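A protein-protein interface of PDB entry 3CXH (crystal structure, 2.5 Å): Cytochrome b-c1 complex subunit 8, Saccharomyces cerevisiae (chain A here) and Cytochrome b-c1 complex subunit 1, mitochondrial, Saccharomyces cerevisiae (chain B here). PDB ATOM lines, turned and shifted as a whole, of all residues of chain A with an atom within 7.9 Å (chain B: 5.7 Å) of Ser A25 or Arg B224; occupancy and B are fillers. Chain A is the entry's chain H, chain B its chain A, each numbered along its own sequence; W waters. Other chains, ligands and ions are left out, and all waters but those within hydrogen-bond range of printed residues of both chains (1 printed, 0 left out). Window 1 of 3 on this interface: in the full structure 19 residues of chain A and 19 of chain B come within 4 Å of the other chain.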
ATOM      1  N   TRP A  12      17.215 -18.569  -8.437  1.00  0.00           N
ATOM      2  CA  TRP A  12      18.192 -19.660  -8.377  1.00  0.00           C
ATOM      3  C   TRP A  12      18.206 -20.342  -7.020  1.00  0.00           C
ATOM      4  O   TRP A  12      18.463 -19.697  -6.011  1.00  0.00           O
ATOM      5  CB  TRP A  12      19.591 -19.135  -8.691  1.00  0.00           C
ATOM      6  CG  TRP A  12      19.695 -18.437 -10.006  1.00  0.00           C
ATOM      7  CD1 TRP A  12      19.871 -17.103 -10.202  1.00  0.00           C
ATOM      8  CD2 TRP A  12      19.667 -19.038 -11.307  1.00  0.00           C
ATOM      9  NE1 TRP A  12      19.956 -16.830 -11.545  1.00  0.00           N
ATOM     10  CE2 TRP A  12      19.836 -18.001 -12.245  1.00  0.00           C
ATOM     11  CE3 TRP A  12      19.524 -20.353 -11.771  1.00  0.00           C
ATOM     12  CZ2 TRP A  12      19.873 -18.236 -13.630  1.00  0.00           C
ATOM     13  CZ3 TRP A  12      19.560 -20.591 -13.146  1.00  0.00           C
ATOM     14  CH2 TRP A  12      19.734 -19.533 -14.057  1.00  0.00           C
ATOM     15  N   GLY A  22      17.047 -38.051 -11.549  1.00  0.00           N
ATOM     16  CA  GLY A  22      17.237 -39.015 -12.619  1.00  0.00           C
ATOM     17  C   GLY A  22      17.713 -38.434 -13.936  1.00  0.00           C
ATOM     18  O   GLY A  22      17.999 -39.174 -14.870  1.00  0.00           O
ATOM     19  N   ILE A  23      17.782 -37.110 -14.023  1.00  0.00           N
ATOM     20  CA  ILE A  23      18.228 -36.448 -15.244  1.00  0.00           C
ATOM     21  C   ILE A  23      19.659 -35.996 -15.082  1.00  0.00           C
ATOM     22  O   ILE A  23      20.015 -35.375 -14.078  1.00  0.00           O
ATOM     23  CB  ILE A  23      17.376 -35.212 -15.569  1.00  0.00           C
ATOM     24  CG1 ILE A  23      15.913 -35.610 -15.737  1.00  0.00           C
ATOM     25  CG2 ILE A  23      17.900 -34.526 -16.828  1.00  0.00           C
ATOM     26  CD1 ILE A  23      14.985 -34.436 -15.793  1.00  0.00           C
ATOM     27  N   THR A  24      20.475 -36.299 -16.080  1.00  0.00           N
ATOM     28  CA  THR A  24      21.870 -35.919 -16.063  1.00  0.00           C
ATOM     29  C   THR A  24      22.151 -35.120 -17.336  1.00  0.00           C
ATOM     30  O   THR A  24      21.641 -35.452 -18.409  1.00  0.00           O
ATOM     31  CB  THR A  24      22.772 -37.184 -15.976  1.00  0.00           C
ATOM     32  OG1 THR A  24      22.582 -37.813 -14.703  1.00  0.00           O
ATOM     33  CG2 THR A  24      24.256 -36.845 -16.151  1.00  0.00           C
ATOM     34  N   SER A  25      22.883 -34.017 -17.192  1.00  0.00           N
ATOM     35  CA  SER A  25      23.235 -33.184 -18.330  1.00  0.00           C
ATOM     36  C   SER A  25      24.753 -33.166 -18.475  1.00  0.00           C
ATOM     37  O   SER A  25      25.485 -33.340 -17.498  1.00  0.00           O
ATOM     38  CB  SER A  25      22.685 -31.749 -18.182  1.00  0.00           C
ATOM     39  OG  SER A  25      23.234 -31.055 -17.070  1.00  0.00           O
ATOM     40  N   TYR A  26      25.214 -33.008 -19.709  1.00  0.00           N
ATOM     41  CA  TYR A  26      26.640 -32.975 -20.006  1.00  0.00           C
ATOM     42  C   TYR A  26      26.848 -31.835 -20.971  1.00  0.00           C
ATOM     43  O   TYR A  26      26.000 -31.582 -21.831  1.00  0.00           O
ATOM     44  CB  TYR A  26      27.084 -34.256 -20.711  1.00  0.00           C
ATOM     45  CG  TYR A  26      26.781 -35.539 -19.995  1.00  0.00           C
ATOM     46  CD1 TYR A  26      25.536 -36.151 -20.122  1.00  0.00           C
ATOM     47  CD2 TYR A  26      27.761 -36.186 -19.256  1.00  0.00           C
ATOM     48  CE1 TYR A  26      25.278 -37.384 -19.531  1.00  0.00           C
ATOM     49  CE2 TYR A  26      27.516 -37.425 -18.661  1.00  0.00           C
ATOM     50  CZ  TYR A  26      26.278 -38.012 -18.805  1.00  0.00           C
ATOM     51  OH  TYR A  26      26.042 -39.238 -18.234  1.00  0.00           O
ATOM     52  N   ALA A  27      27.980 -31.160 -20.846  1.00  0.00           N
ATOM     53  CA  ALA A  27      28.277 -30.054 -21.727  1.00  0.00           C
ATOM     54  C   ALA A  27      29.769 -29.947 -21.877  1.00  0.00           C
ATOM     55  O   ALA A  27      30.518 -30.380 -21.002  1.00  0.00           O
ATOM     56  CB  ALA A  27      27.714 -28.745 -21.166  1.00  0.00           C
ATOM     57  N   GLU B 222      31.659 -30.463 -18.166  1.00  0.00           N
ATOM     58  CA  GLU B 222      30.926 -30.623 -16.919  1.00  0.00           C
ATOM     59  C   GLU B 222      29.896 -31.739 -17.022  1.00  0.00           C
ATOM     60  O   GLU B 222      29.459 -32.103 -18.119  1.00  0.00           O
ATOM     61  CB  GLU B 222      30.181 -29.330 -16.580  1.00  0.00           C
ATOM     62  CG  GLU B 222      29.060 -29.002 -17.570  1.00  0.00           C
ATOM     63  CD  GLU B 222      28.246 -27.779 -17.185  1.00  0.00           C
ATOM     64  OE1 GLU B 222      27.018 -27.786 -17.419  1.00  0.00           O
ATOM     65  OE2 GLU B 222      28.828 -26.809 -16.659  1.00  0.00           O
ATOM     66  N   VAL B 223      29.516 -32.272 -15.863  1.00  0.00           N
ATOM     67  CA  VAL B 223      28.496 -33.304 -15.769  1.00  0.00           C
ATOM     68  C   VAL B 223      27.658 -32.948 -14.534  1.00  0.00           C
ATOM     69  O   VAL B 223      28.190 -32.736 -13.441  1.00  0.00           O
ATOM     70  CB  VAL B 223      29.106 -34.742 -15.687  1.00  0.00           C
ATOM     71  CG1 VAL B 223      30.033 -34.873 -14.510  1.00  0.00           C
ATOM     72  CG2 VAL B 223      27.998 -35.792 -15.625  1.00  0.00           C
ATOM     73  N   ARG B 224      26.351 -32.819 -14.730  1.00  0.00           N
ATOM     74  CA  ARG B 224      25.448 -32.444 -13.641  1.00  0.00           C
ATOM     75  C   ARG B 224      24.438 -33.522 -13.277  1.00  0.00           C
ATOM     76  O   ARG B 224      23.561 -33.854 -14.080  1.00  0.00           O
ATOM     77  CB  ARG B 224      24.706 -31.152 -13.997  1.00  0.00           C
ATOM     78  CG  ARG B 224      25.610 -29.954 -14.247  1.00  0.00           C
ATOM     79  CD  ARG B 224      24.820 -28.749 -14.744  1.00  0.00           C
ATOM     80  NE  ARG B 224      25.704 -27.622 -14.995  1.00  0.00           N
ATOM     81  CZ  ARG B 224      25.748 -26.516 -14.256  1.00  0.00           C
ATOM     82  NH1 ARG B 224      26.606 -25.557 -14.569  1.00  0.00           N
ATOM     83  NH2 ARG B 224      24.918 -26.357 -13.230  1.00  0.00           N
ATOM     84  N   LEU B 225      24.576 -34.057 -12.061  1.00  0.00           N
ATOM     85  CA  LEU B 225      23.688 -35.095 -11.537  1.00  0.00           C
ATOM     86  C   LEU B 225      22.696 -34.447 -10.562  1.00  0.00           C
ATOM     87  O   LEU B 225      22.729 -34.737  -9.366  1.00  0.00           O
ATOM     88  CB  LEU B 225      24.488 -36.171 -10.776  1.00  0.00           C
ATOM     89  CG  LEU B 225      25.543 -37.135 -11.349  1.00  0.00           C
ATOM     90  CD1 LEU B 225      25.031 -37.794 -12.604  1.00  0.00           C
ATOM     91  CD2 LEU B 225      26.846 -36.434 -11.618  1.00  0.00           C
ATOM     92  N   ARG B 226      21.823 -33.572 -11.058  1.00  0.00           N
ATOM     93  CA  ARG B 226      20.872 -32.904 -10.169  1.00  0.00           C
ATOM     94  C   ARG B 226      19.890 -33.856  -9.516  1.00  0.00           C
ATOM     95  O   ARG B 226      19.287 -34.683 -10.182  1.00  0.00           O
ATOM     96  CB  ARG B 226      20.086 -31.793 -10.877  1.00  0.00           C
ATOM     97  CG  ARG B 226      19.688 -30.668  -9.905  1.00  0.00           C
ATOM     98  CD  ARG B 226      18.231 -30.214  -9.992  1.00  0.00           C
ATOM     99  NE  ARG B 226      18.075 -29.007 -10.797  1.00  0.00           N
ATOM    100  CZ  ARG B 226      17.100 -28.106 -10.652  1.00  0.00           C
ATOM    101  NH1 ARG B 226      17.060 -27.055 -11.459  1.00  0.00           N
ATOM    102  NH2 ARG B 226      16.171 -28.238  -9.714  1.00  0.00           N
ATOM    103  N   ILE B 407      33.709 -29.537 -14.343  1.00  0.00           N
ATOM    104  CA  ILE B 407      32.776 -29.419 -13.230  1.00  0.00           C
ATOM    105  C   ILE B 407      31.911 -30.664 -13.094  1.00  0.00           C
ATOM    106  O   ILE B 407      31.498 -31.261 -14.086  1.00  0.00           O
ATOM    107  CB  ILE B 407      31.805 -28.210 -13.411  1.00  0.00           C
ATOM    108  CG1 ILE B 407      32.576 -26.935 -13.732  1.00  0.00           C
ATOM    109  CG2 ILE B 407      30.968 -28.016 -12.154  1.00  0.00           C
ATOM    110  CD1 ILE B 407      31.683 -25.788 -14.187  1.00  0.00           C
ATOM    111  N   ALA B 408      31.599 -31.009 -11.853  1.00  0.00           N
ATOM    112  CA  ALA B 408      30.750 -32.149 -11.549  1.00  0.00           C
ATOM    113  C   ALA B 408      29.991 -31.796 -10.274  1.00  0.00           C
ATOM    114  O   ALA B 408      30.510 -31.090  -9.407  1.00  0.00           O
ATOM    115  CB  ALA B 408      31.581 -33.391 -11.339  1.00  0.00           C
ATOM    116  N   GLY B 409      28.749 -32.253 -10.181  1.00  0.00           N
ATOM    117  CA  GLY B 409      27.964 -31.954  -9.002  1.00  0.00           C
ATOM    118  C   GLY B 409      26.687 -32.749  -8.913  1.00  0.00           C
ATOM    119  O   GLY B 409      26.172 -33.231  -9.927  1.00  0.00           O
ATOM    120  N   ILE B 413      21.619 -28.633  -7.011  1.00  0.00           N
ATOM    121  CA  ILE B 413      22.510 -27.772  -7.769  1.00  0.00           C
ATOM    122  C   ILE B 413      21.839 -26.801  -8.734  1.00  0.00           C
ATOM    123  O   ILE B 413      22.482 -26.299  -9.664  1.00  0.00           O
ATOM    124  CB  ILE B 413      23.600 -28.592  -8.507  1.00  0.00           C
ATOM    125  CG1 ILE B 413      22.968 -29.729  -9.305  1.00  0.00           C
ATOM    126  CG2 ILE B 413      24.615 -29.148  -7.515  1.00  0.00           C
ATOM    127  CD1 ILE B 413      23.909 -30.358 -10.297  1.00  0.00           C
ATOM    128  N   LEU B 416      23.761 -23.647  -9.169  1.00  0.00           N
ATOM    129  CA  LEU B 416      25.088 -23.654  -9.800  1.00  0.00           C
ATOM    130  C   LEU B 416      24.912 -23.152 -11.231  1.00  0.00           C
ATOM    131  O   LEU B 416      24.325 -23.825 -12.077  1.00  0.00           O
ATOM    132  CB  LEU B 416      25.695 -25.059  -9.774  1.00  0.00           C
ATOM    133  CG  LEU B 416      27.090 -25.272 -10.376  1.00  0.00           C
ATOM    134  CD1 LEU B 416      28.151 -24.506  -9.611  1.00  0.00           C
ATOM    135  CD2 LEU B 416      27.417 -26.764 -10.389  1.00  0.00           C
ATOM    136  N   LEU B 417      25.343 -21.920 -11.470  1.00  0.00           N
ATOM    137  CA  LEU B 417      25.219 -21.293 -12.781  1.00  0.00           C
ATOM    138  C   LEU B 417      25.861 -22.070 -13.926  1.00  0.00           C
ATOM    139  O   LEU B 417      26.678 -22.956 -13.703  1.00  0.00           O
ATOM    140  CB  LEU B 417      25.796 -19.879 -12.721  1.00  0.00           C
ATOM    141  CG  LEU B 417      24.828 -18.757 -12.333  1.00  0.00           C
ATOM    142  CD1 LEU B 417      23.764 -19.249 -11.363  1.00  0.00           C
ATOM    143  CD2 LEU B 417      25.611 -17.586 -11.769  1.00  0.00           C
ATOM    144  N   ASP B 418      25.479 -21.720 -15.150  1.00  0.00           N
ATOM    145  CA  ASP B 418      26.001 -22.341 -16.369  1.00  0.00           C
ATOM    146  C   ASP B 418      27.532 -22.361 -16.431  1.00  0.00           C
ATOM    147  O   ASP B 418      28.204 -21.529 -15.813  1.00  0.00           O
ATOM    148  CB  ASP B 418      25.513 -21.556 -17.567  1.00  0.00           C
ATOM    149  CG  ASP B 418      25.965 -20.125 -17.516  1.00  0.00           C
ATOM    150  OD1 ASP B 418      25.346 -19.355 -16.759  1.00  0.00           O
ATOM    151  OD2 ASP B 418      26.963 -19.776 -18.183  1.00  0.00           O
ATOM    152  N   TYR B 419      28.057 -23.228 -17.295  1.00  0.00           N
ATOM    153  CA  TYR B 419      29.500 -23.391 -17.476  1.00  0.00           C
ATOM    154  C   TYR B 419      30.212 -22.074 -17.721  1.00  0.00           C
ATOM    155  O   TYR B 419      31.138 -21.719 -16.987  1.00  0.00           O
ATOM    156  CB  TYR B 419      29.787 -24.356 -18.635  1.00  0.00           C
ATOM    157  CG  TYR B 419      31.249 -24.704 -18.802  1.00  0.00           C
ATOM    158  CD1 TYR B 419      31.814 -25.767 -18.097  1.00  0.00           C
ATOM    159  CD2 TYR B 419      32.075 -23.952 -19.639  1.00  0.00           C
ATOM    160  CE1 TYR B 419      33.167 -26.073 -18.214  1.00  0.00           C
ATOM    161  CE2 TYR B 419      33.431 -24.243 -19.761  1.00  0.00           C
ATOM    162  CZ  TYR B 419      33.974 -25.306 -19.040  1.00  0.00           C
ATOM    163  OH  TYR B 419      35.328 -25.567 -19.109  1.00  0.00           O
ATOM    164  N   ILE B 422      30.764 -19.709 -14.714  1.00  0.00           N
ATOM    165  CA  ILE B 422      31.815 -20.224 -13.840  1.00  0.00           C
ATOM    166  C   ILE B 422      33.148 -19.997 -14.550  1.00  0.00           C
ATOM    167  O   ILE B 422      34.085 -19.448 -13.971  1.00  0.00           O
ATOM    168  CB  ILE B 422      31.664 -21.747 -13.562  1.00  0.00           C
ATOM    169  CG1 ILE B 422      30.223 -22.119 -13.207  1.00  0.00           C
ATOM    170  CG2 ILE B 422      32.561 -22.159 -12.428  1.00  0.00           C
ATOM    171  CD1 ILE B 422      29.638 -21.339 -12.080  1.00  0.00           C
HETATM  172  O   HOH W   1      17.582 -34.647 -12.374  1.00  0.00           O
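Arg B224 touches just these residues of chain A: Ile A23 (3.9 Å), Thr A24 (3.3 Å) and Ser A25 (2.9 Å).
Of the printed residues of chain A, Leu B225 touches Thr A24 (3.2 Å).
Of the printed residues of chain A, Val B223 touches Thr A24 (3.9 Å), Ser A25 (3.5 Å) and Tyr A26 (3.5 Å).
Of the printed residues of chain B, Thr A24 touches Val B223 (3.9 Å), Arg B224 (3.3 Å) and Leu B225 (3.2 Å).
Asp B418 touches none of the printed residues of chain A.
Ala B408 touches none of the printed residues of chain A.
The nearest residue of chain B that does not touch Ser A25 is Glu B222 (4.2 Å).
The nearest residue of chain A that does not touch Arg B224 is Tyr A26 (5.1 Å).
The backbone NH of Gly B409 sits at hydrogen-bond distance from the backbone carbonyl oxygen of Val B223, at 3.3 Å.
N of Leu B225 is in hydrogen-bond range of O of Gly B409, 2.8 Å away.
NE of Arg B224 is in salt-bridge range of OE1 of Glu B222 (2.8 Å).
The backbone NH (N) of Val B223 is in hydrogen-bond range of the backbone carbonyl oxygen (O) of Ile B407, at 2.8 Å.
O of Leu B416 lies within hydrogen-bond range of NH2 of Arg B224 (2.8 Å).
The backbone carbonyl oxygen of Leu B417 lies within hydrogen-bond range of the guanidinium group of Arg B224.
Of the 7 printed residues of chain A, 5 touch a printed residue of chain B.
Hydrophobic or aromatic side chains of chain A that line the printed part of chain B: Tyr A26 and Ala A27.
Among the printed residues, no Asp or Glu carboxylate lies within 4 Å of a Lys or Arg side-chain nitrogen of the other chain.
Water W1 lies within hydrogen-bond range of the backbone carbonyl oxygen (O) of Arg B226 (2.8 Å) and the backbone NH (N) of Ile A23 (3.0 Å).
Among the printed residues, pairs that only touch across the chains: Ile A23 with Arg B224, Ile A23 with Arg B226, Thr A24 with Val B223, Thr A24 with Arg B224, Thr A24 with Leu B225, Ser A25 with Val B223, Tyr A26 with Glu B222 and Tyr A26 with Val B223.
The backbone NH of Arg B224 sits at hydrogen-bond distance from the backbone carbonyl oxygen of Ser A25.
O of Ala A27 sits at hydrogen-bond distance from N of Glu B222 (3.1 Å).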
